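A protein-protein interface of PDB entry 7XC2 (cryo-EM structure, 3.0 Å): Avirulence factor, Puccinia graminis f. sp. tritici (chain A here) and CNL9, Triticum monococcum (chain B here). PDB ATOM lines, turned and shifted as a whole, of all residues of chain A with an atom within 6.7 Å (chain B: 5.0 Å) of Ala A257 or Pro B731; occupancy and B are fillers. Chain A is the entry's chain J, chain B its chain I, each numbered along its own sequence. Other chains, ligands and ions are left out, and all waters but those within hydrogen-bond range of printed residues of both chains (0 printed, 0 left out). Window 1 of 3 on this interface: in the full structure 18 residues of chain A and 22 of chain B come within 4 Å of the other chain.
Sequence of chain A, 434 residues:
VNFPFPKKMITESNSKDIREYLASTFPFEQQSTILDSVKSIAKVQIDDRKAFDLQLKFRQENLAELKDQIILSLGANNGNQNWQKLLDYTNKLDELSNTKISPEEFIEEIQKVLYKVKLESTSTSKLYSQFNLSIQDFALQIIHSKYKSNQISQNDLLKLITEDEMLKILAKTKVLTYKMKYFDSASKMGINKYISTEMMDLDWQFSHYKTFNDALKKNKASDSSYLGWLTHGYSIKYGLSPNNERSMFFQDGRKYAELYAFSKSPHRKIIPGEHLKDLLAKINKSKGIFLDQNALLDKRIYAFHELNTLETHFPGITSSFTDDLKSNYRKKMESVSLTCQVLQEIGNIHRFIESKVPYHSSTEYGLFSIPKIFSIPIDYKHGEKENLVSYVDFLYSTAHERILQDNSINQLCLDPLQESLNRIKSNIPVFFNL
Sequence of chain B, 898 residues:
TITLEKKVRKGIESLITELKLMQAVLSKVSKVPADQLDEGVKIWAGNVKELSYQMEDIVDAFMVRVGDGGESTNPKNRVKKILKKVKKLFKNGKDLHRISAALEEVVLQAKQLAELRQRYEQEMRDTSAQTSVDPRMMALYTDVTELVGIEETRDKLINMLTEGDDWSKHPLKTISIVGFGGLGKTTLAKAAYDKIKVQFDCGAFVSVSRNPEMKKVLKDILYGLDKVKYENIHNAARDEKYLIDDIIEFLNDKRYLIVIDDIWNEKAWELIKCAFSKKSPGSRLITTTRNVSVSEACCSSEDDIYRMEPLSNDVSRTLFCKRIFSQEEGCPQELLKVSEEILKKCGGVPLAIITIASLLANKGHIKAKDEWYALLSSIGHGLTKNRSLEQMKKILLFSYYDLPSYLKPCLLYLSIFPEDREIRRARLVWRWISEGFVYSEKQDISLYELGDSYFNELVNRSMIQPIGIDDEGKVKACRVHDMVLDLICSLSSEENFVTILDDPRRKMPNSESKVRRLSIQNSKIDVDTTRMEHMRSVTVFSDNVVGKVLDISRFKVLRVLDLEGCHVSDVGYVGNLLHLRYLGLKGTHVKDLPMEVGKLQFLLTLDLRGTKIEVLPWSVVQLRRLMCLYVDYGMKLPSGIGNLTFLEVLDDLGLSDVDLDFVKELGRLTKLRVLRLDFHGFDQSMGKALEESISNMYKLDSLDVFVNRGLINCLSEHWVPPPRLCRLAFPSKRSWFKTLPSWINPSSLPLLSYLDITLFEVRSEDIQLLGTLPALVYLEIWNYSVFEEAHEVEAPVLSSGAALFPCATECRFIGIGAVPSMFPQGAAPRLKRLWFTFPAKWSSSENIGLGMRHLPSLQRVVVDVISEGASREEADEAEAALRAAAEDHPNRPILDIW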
ATOM      1  N   TRP A 229      -1.446 -20.121  23.661  1.00  0.00           N
ATOM      2  CA  TRP A 229      -1.522 -21.420  23.009  1.00  0.00           C
ATOM      3  C   TRP A 229      -2.059 -22.480  23.954  1.00  0.00           C
ATOM      4  O   TRP A 229      -2.657 -23.465  23.509  1.00  0.00           O
ATOM      5  CB  TRP A 229      -0.147 -21.820  22.481  1.00  0.00           C
ATOM      6  CG  TRP A 229      -0.098 -23.176  21.863  1.00  0.00           C
ATOM      7  CD1 TRP A 229      -0.304 -23.485  20.557  1.00  0.00           C
ATOM      8  CD2 TRP A 229       0.190 -24.405  22.527  1.00  0.00           C
ATOM      9  NE1 TRP A 229      -0.168 -24.835  20.364  1.00  0.00           N
ATOM     10  CE2 TRP A 229       0.136 -25.422  21.563  1.00  0.00           C
ATOM     11  CE3 TRP A 229       0.483 -24.747  23.846  1.00  0.00           C
ATOM     12  CZ2 TRP A 229       0.364 -26.753  21.873  1.00  0.00           C
ATOM     13  CZ3 TRP A 229       0.710 -26.066  24.151  1.00  0.00           C
ATOM     14  CH2 TRP A 229       0.649 -27.053  23.172  1.00  0.00           C
ATOM     15  N   ASP A 252      -0.869 -31.007  21.548  1.00  0.00           N
ATOM     16  CA  ASP A 252       0.387 -31.738  21.564  1.00  0.00           C
ATOM     17  C   ASP A 252       1.521 -30.848  22.049  1.00  0.00           C
ATOM     18  O   ASP A 252       1.603 -29.673  21.685  1.00  0.00           O
ATOM     19  CB  ASP A 252       0.710 -32.277  20.173  1.00  0.00           C
ATOM     20  CG  ASP A 252       1.808 -33.310  20.195  1.00  0.00           C
ATOM     21  OD1 ASP A 252       2.300 -33.630  21.296  1.00  0.00           O
ATOM     22  OD2 ASP A 252       2.183 -33.805  19.114  1.00  0.00           O
ATOM     23  N   GLY A 253       2.403 -31.423  22.865  1.00  0.00           N
ATOM     24  CA  GLY A 253       3.515 -30.653  23.389  1.00  0.00           C
ATOM     25  C   GLY A 253       4.579 -30.368  22.348  1.00  0.00           C
ATOM     26  O   GLY A 253       5.202 -29.305  22.364  1.00  0.00           O
ATOM     27  N   ARG A 254       4.802 -31.304  21.430  1.00  0.00           N
ATOM     28  CA  ARG A 254       5.868 -31.118  20.453  1.00  0.00           C
ATOM     29  C   ARG A 254       5.516 -30.122  19.366  1.00  0.00           C
ATOM     30  O   ARG A 254       6.356 -29.866  18.501  1.00  0.00           O
ATOM     31  CB  ARG A 254       6.241 -32.448  19.807  1.00  0.00           C
ATOM     32  CG  ARG A 254       6.759 -33.474  20.780  1.00  0.00           C
ATOM     33  CD  ARG A 254       7.734 -34.420  20.118  1.00  0.00           C
ATOM     34  NE  ARG A 254       8.189 -35.451  21.043  1.00  0.00           N
ATOM     35  CZ  ARG A 254       9.366 -36.055  20.964  1.00  0.00           C
ATOM     36  NH1 ARG A 254      10.218 -35.723  20.007  1.00  0.00           N
ATOM     37  NH2 ARG A 254       9.697 -36.982  21.848  1.00  0.00           N
ATOM     38  N   LYS A 255       4.313 -29.560  19.370  1.00  0.00           N
ATOM     39  CA  LYS A 255       3.982 -28.525  18.402  1.00  0.00           C
ATOM     40  C   LYS A 255       4.402 -27.150  18.892  1.00  0.00           C
ATOM     41  O   LYS A 255       4.885 -26.325  18.105  1.00  0.00           O
ATOM     42  CB  LYS A 255       2.483 -28.533  18.114  1.00  0.00           C
ATOM     43  CG  LYS A 255       1.953 -29.877  17.683  1.00  0.00           C
ATOM     44  CD  LYS A 255       2.638 -30.348  16.423  1.00  0.00           C
ATOM     45  CE  LYS A 255       2.074 -31.676  15.970  1.00  0.00           C
ATOM     46  NZ  LYS A 255       0.593 -31.653  15.971  1.00  0.00           N
ATOM     47  N   TYR A 256       4.223 -26.891  20.186  1.00  0.00           N
ATOM     48  CA  TYR A 256       4.672 -25.625  20.737  1.00  0.00           C
ATOM     49  C   TYR A 256       6.175 -25.461  20.588  1.00  0.00           C
ATOM     50  O   TYR A 256       6.658 -24.343  20.395  1.00  0.00           O
ATOM     51  CB  TYR A 256       4.281 -25.510  22.202  1.00  0.00           C
ATOM     52  CG  TYR A 256       4.841 -24.271  22.833  1.00  0.00           C
ATOM     53  CD1 TYR A 256       4.310 -23.030  22.540  1.00  0.00           C
ATOM     54  CD2 TYR A 256       5.914 -24.333  23.698  1.00  0.00           C
ATOM     55  CE1 TYR A 256       4.820 -21.893  23.100  1.00  0.00           C
ATOM     56  CE2 TYR A 256       6.432 -23.200  24.263  1.00  0.00           C
ATOM     57  CZ  TYR A 256       5.881 -21.981  23.961  1.00  0.00           C
ATOM     58  OH  TYR A 256       6.395 -20.841  24.525  1.00  0.00           O
ATOM     59  N   ALA A 257       6.927 -26.557  20.676  1.00  0.00           N
ATOM     60  CA  ALA A 257       8.369 -26.468  20.489  1.00  0.00           C
ATOM     61  C   ALA A 257       8.702 -25.971  19.093  1.00  0.00           C
ATOM     62  O   ALA A 257       9.551 -25.088  18.919  1.00  0.00           O
ATOM     63  CB  ALA A 257       9.015 -27.825  20.747  1.00  0.00           C
ATOM     64  N   GLU A 258       8.035 -26.521  18.082  1.00  0.00           N
ATOM     65  CA  GLU A 258       8.288 -26.089  16.713  1.00  0.00           C
ATOM     66  C   GLU A 258       7.888 -24.637  16.516  1.00  0.00           C
ATOM     67  O   GLU A 258       8.604 -23.869  15.860  1.00  0.00           O
ATOM     68  CB  GLU A 258       7.534 -26.988  15.739  1.00  0.00           C
ATOM     69  CG  GLU A 258       8.262 -27.235  14.444  1.00  0.00           C
ATOM     70  CD  GLU A 258       9.517 -28.059  14.632  1.00  0.00           C
ATOM     71  OE1 GLU A 258       9.567 -28.858  15.588  1.00  0.00           O
ATOM     72  OE2 GLU A 258      10.453 -27.912  13.820  1.00  0.00           O
ATOM     73  N   LEU A 259       6.749 -24.241  17.084  1.00  0.00           N
ATOM     74  CA  LEU A 259       6.313 -22.858  16.942  1.00  0.00           C
ATOM     75  C   LEU A 259       7.306 -21.901  17.585  1.00  0.00           C
ATOM     76  O   LEU A 259       7.648 -20.867  17.005  1.00  0.00           O
ATOM     77  CB  LEU A 259       4.923 -22.681  17.543  1.00  0.00           C
ATOM     78  CG  LEU A 259       3.826 -23.411  16.775  1.00  0.00           C
ATOM     79  CD1 LEU A 259       2.465 -23.081  17.339  1.00  0.00           C
ATOM     80  CD2 LEU A 259       3.888 -23.057  15.310  1.00  0.00           C
ATOM     81  N   TYR A 260       7.795 -22.239  18.777  1.00  0.00           N
ATOM     82  CA  TYR A 260       8.785 -21.396  19.437  1.00  0.00           C
ATOM     83  C   TYR A 260      10.065 -21.311  18.622  1.00  0.00           C
ATOM     84  O   TYR A 260      10.628 -20.223  18.443  1.00  0.00           O
ATOM     85  CB  TYR A 260       9.072 -21.945  20.831  1.00  0.00           C
ATOM     86  CG  TYR A 260      10.140 -21.204  21.589  1.00  0.00           C
ATOM     87  CD1 TYR A 260      11.478 -21.526  21.438  1.00  0.00           C
ATOM     88  CD2 TYR A 260       9.809 -20.196  22.474  1.00  0.00           C
ATOM     89  CE1 TYR A 260      12.452 -20.856  22.132  1.00  0.00           C
ATOM     90  CE2 TYR A 260      10.777 -19.522  23.174  1.00  0.00           C
ATOM     91  CZ  TYR A 260      12.096 -19.855  22.999  1.00  0.00           C
ATOM     92  OH  TYR A 260      13.066 -19.183  23.696  1.00  0.00           O
ATOM     93  N   ALA A 261      10.548 -22.453  18.132  1.00  0.00           N
ATOM     94  CA  ALA A 261      11.758 -22.454  17.320  1.00  0.00           C
ATOM     95  C   ALA A 261      11.609 -21.533  16.121  1.00  0.00           C
ATOM     96  O   ALA A 261      12.514 -20.749  15.818  1.00  0.00           O
ATOM     97  CB  ALA A 261      12.087 -23.873  16.868  1.00  0.00           C
ATOM     98  N   PHE A 262      10.470 -21.600  15.433  1.00  0.00           N
ATOM     99  CA  PHE A 262      10.241 -20.674  14.331  1.00  0.00           C
ATOM    100  C   PHE A 262      10.215 -19.236  14.823  1.00  0.00           C
ATOM    101  O   PHE A 262      10.740 -18.334  14.162  1.00  0.00           O
ATOM    102  CB  PHE A 262       8.936 -21.002  13.617  1.00  0.00           C
ATOM    103  CG  PHE A 262       8.344 -19.837  12.882  1.00  0.00           C
ATOM    104  CD1 PHE A 262       8.797 -19.500  11.624  1.00  0.00           C
ATOM    105  CD2 PHE A 262       7.339 -19.078  13.449  1.00  0.00           C
ATOM    106  CE1 PHE A 262       8.262 -18.432  10.945  1.00  0.00           C
ATOM    107  CE2 PHE A 262       6.802 -18.007  12.774  1.00  0.00           C
ATOM    108  CZ  PHE A 262       7.263 -17.684  11.521  1.00  0.00           C
ATOM    109  N   ARG A 268      13.624 -20.677   9.405  1.00  0.00           N
ATOM    110  CA  ARG A 268      13.205 -22.071   9.363  1.00  0.00           C
ATOM    111  C   ARG A 268      12.041 -22.273   8.410  1.00  0.00           C
ATOM    112  O   ARG A 268      11.922 -23.338   7.795  1.00  0.00           O
ATOM    113  CB  ARG A 268      12.817 -22.541  10.760  1.00  0.00           C
ATOM    114  CG  ARG A 268      13.981 -22.700  11.699  1.00  0.00           C
ATOM    115  CD  ARG A 268      13.608 -23.580  12.866  1.00  0.00           C
ATOM    116  NE  ARG A 268      14.753 -24.346  13.336  1.00  0.00           N
ATOM    117  CZ  ARG A 268      14.659 -25.462  14.046  1.00  0.00           C
ATOM    118  NH1 ARG A 268      13.468 -25.944  14.367  1.00  0.00           N
ATOM    119  NH2 ARG A 268      15.755 -26.096  14.431  1.00  0.00           N
ATOM    120  N   VAL B 705      15.098 -37.168  23.579  1.00  0.00           N
ATOM    121  CA  VAL B 705      14.613 -36.759  24.883  1.00  0.00           C
ATOM    122  C   VAL B 705      13.908 -35.430  24.702  1.00  0.00           C
ATOM    123  O   VAL B 705      14.527 -34.451  24.274  1.00  0.00           O
ATOM    124  CB  VAL B 705      15.741 -36.627  25.914  1.00  0.00           C
ATOM    125  CG1 VAL B 705      15.168 -36.189  27.234  1.00  0.00           C
ATOM    126  CG2 VAL B 705      16.479 -37.934  26.068  1.00  0.00           C
ATOM    127  N   PHE B 706      12.626 -35.390  25.023  1.00  0.00           N
ATOM    128  CA  PHE B 706      11.844 -34.170  24.935  1.00  0.00           C
ATOM    129  C   PHE B 706      11.524 -33.695  26.340  1.00  0.00           C
ATOM    130  O   PHE B 706      11.045 -34.476  27.163  1.00  0.00           O
ATOM    131  CB  PHE B 706      10.564 -34.402  24.141  1.00  0.00           C
ATOM    132  CG  PHE B 706       9.695 -33.201  24.049  1.00  0.00           C
ATOM    133  CD1 PHE B 706      10.004 -32.178  23.183  1.00  0.00           C
ATOM    134  CD2 PHE B 706       8.564 -33.092  24.824  1.00  0.00           C
ATOM    135  CE1 PHE B 706       9.204 -31.069  23.096  1.00  0.00           C
ATOM    136  CE2 PHE B 706       7.762 -31.987  24.738  1.00  0.00           C
ATOM    137  CZ  PHE B 706       8.081 -30.974  23.873  1.00  0.00           C
ATOM    138  N   ALA B 729      19.348 -36.301  19.678  1.00  0.00           N
ATOM    139  CA  ALA B 729      18.599 -35.070  19.491  1.00  0.00           C
ATOM    140  C   ALA B 729      17.819 -34.724  20.748  1.00  0.00           C
ATOM    141  O   ALA B 729      17.267 -35.605  21.407  1.00  0.00           O
ATOM    142  CB  ALA B 729      17.642 -35.188  18.305  1.00  0.00           C
ATOM    143  N   PHE B 730      17.778 -33.433  21.064  1.00  0.00           N
ATOM    144  CA  PHE B 730      16.939 -32.889  22.130  1.00  0.00           C
ATOM    145  C   PHE B 730      16.152 -31.741  21.521  1.00  0.00           C
ATOM    146  O   PHE B 730      16.596 -30.587  21.550  1.00  0.00           O
ATOM    147  CB  PHE B 730      17.768 -32.415  23.316  1.00  0.00           C
ATOM    148  CG  PHE B 730      18.666 -33.464  23.889  1.00  0.00           C
ATOM    149  CD1 PHE B 730      19.926 -33.670  23.372  1.00  0.00           C
ATOM    150  CD2 PHE B 730      18.255 -34.234  24.955  1.00  0.00           C
ATOM    151  CE1 PHE B 730      20.752 -34.631  23.901  1.00  0.00           C
ATOM    152  CE2 PHE B 730      19.079 -35.194  25.486  1.00  0.00           C
ATOM    153  CZ  PHE B 730      20.329 -35.392  24.957  1.00  0.00           C
ATOM    154  N   PRO B 731      14.982 -32.010  20.975  1.00  0.00           N
ATOM    155  CA  PRO B 731      14.267 -30.980  20.216  1.00  0.00           C
ATOM    156  C   PRO B 731      13.510 -29.998  21.090  1.00  0.00           C
ATOM    157  O   PRO B 731      12.627 -29.291  20.600  1.00  0.00           O
ATOM    158  CB  PRO B 731      13.305 -31.800  19.356  1.00  0.00           C
ATOM    159  CG  PRO B 731      13.030 -32.992  20.178  1.00  0.00           C
ATOM    160  CD  PRO B 731      14.294 -33.308  20.921  1.00  0.00           C
ATOM    161  N   SER B 732      13.835 -29.948  22.379  1.00  0.00           N
ATOM    162  CA  SER B 732      13.084 -29.107  23.304  1.00  0.00           C
ATOM    163  C   SER B 732      13.165 -27.635  22.918  1.00  0.00           C
ATOM    164  O   SER B 732      12.139 -26.979  22.708  1.00  0.00           O
ATOM    165  CB  SER B 732      13.599 -29.319  24.722  1.00  0.00           C
ATOM    166  OG  SER B 732      12.914 -28.478  25.632  1.00  0.00           O
ATOM    167  N   LYS B 733      14.382 -27.095  22.843  1.00  0.00           N
ATOM    168  CA  LYS B 733      14.714 -25.705  22.524  1.00  0.00           C
ATOM    169  C   LYS B 733      14.365 -24.732  23.637  1.00  0.00           C
ATOM    170  O   LYS B 733      14.656 -23.541  23.505  1.00  0.00           O
ATOM    171  CB  LYS B 733      14.050 -25.205  21.235  1.00  0.00           C
ATOM    172  CG  LYS B 733      14.372 -26.031  20.024  1.00  0.00           C
ATOM    173  CD  LYS B 733      15.835 -25.925  19.683  1.00  0.00           C
ATOM    174  CE  LYS B 733      16.153 -26.736  18.448  1.00  0.00           C
ATOM    175  NZ  LYS B 733      16.993 -27.914  18.772  1.00  0.00           N
ATOM    176  N   ASP B 756      21.939 -32.196  18.081  1.00  0.00           N
ATOM    177  CA  ASP B 756      21.032 -31.059  18.190  1.00  0.00           C
ATOM    178  C   ASP B 756      20.885 -30.744  19.674  1.00  0.00           C
ATOM    179  O   ASP B 756      20.182 -31.459  20.389  1.00  0.00           O
ATOM    180  CB  ASP B 756      19.692 -31.382  17.549  1.00  0.00           C
ATOM    181  CG  ASP B 756      18.736 -30.219  17.582  1.00  0.00           C
ATOM    182  OD1 ASP B 756      19.134 -29.128  18.037  1.00  0.00           O
ATOM    183  OD2 ASP B 756      17.579 -30.392  17.147  1.00  0.00           O
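The backbone NH (N) of Arg A254 lies close to the side-chain carboxylate (OD1) of Asp A252 (3.4 Å).
The side-chain amino group (NZ) of Lys B733 lies within salt-bridge range of the side-chain carboxylate (OD1) of Asp B756.
Gly A253 touches Phe B706.
Arg A254 touches Phe B706 (NH2 to CB, 3.6 Å).
NH1 of Arg A254 touches CG of Pro B731 (3.9 Å).
Ala A257 touches Pro B731 (CB to O, 3.9 Å).
Ser B732 touches Ala A257 (O to CB, 3.8 Å).
Tyr A260 touches Lys B733 (CE1 to O, 3.7 Å).
Printed residues of chain B within 4 Å of Ala A257: Pro B731 (3.9 Å) and Ser B732 (3.8 Å).
Of chain A, only Arg A254 (3.9 Å) and Ala A257 (3.9 Å) come within 4 Å of Pro B731.
Printed residues of chain A within 4 Å of Lys B733: Tyr A260 (3.7 Å).
Printed residues of chain A within 4 Å of Phe B706: Gly A253 and Arg A254.
Printed residues of chain A within 4 Å of Ser B732: Ala A257 (3.8 Å).
Of the printed residues of chain B, Arg A254 touches Phe B706 (3.6 Å) and Pro B731 (3.9 Å).
Of the printed residues of chain B, Tyr A260 touches Lys B733.
Arg A268 touches none of the printed residues of chain B.
Ala A261 touches none of the printed residues of chain B.
The nearest printed residue of chain A that does not touch Phe B706 is Ala A257 (4.01 Å).
Of the 13 printed residues of chain A, 4 touch a printed residue of chain B.
Of the 8 printed residues of chain B, 4 touch a printed residue of chain A.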
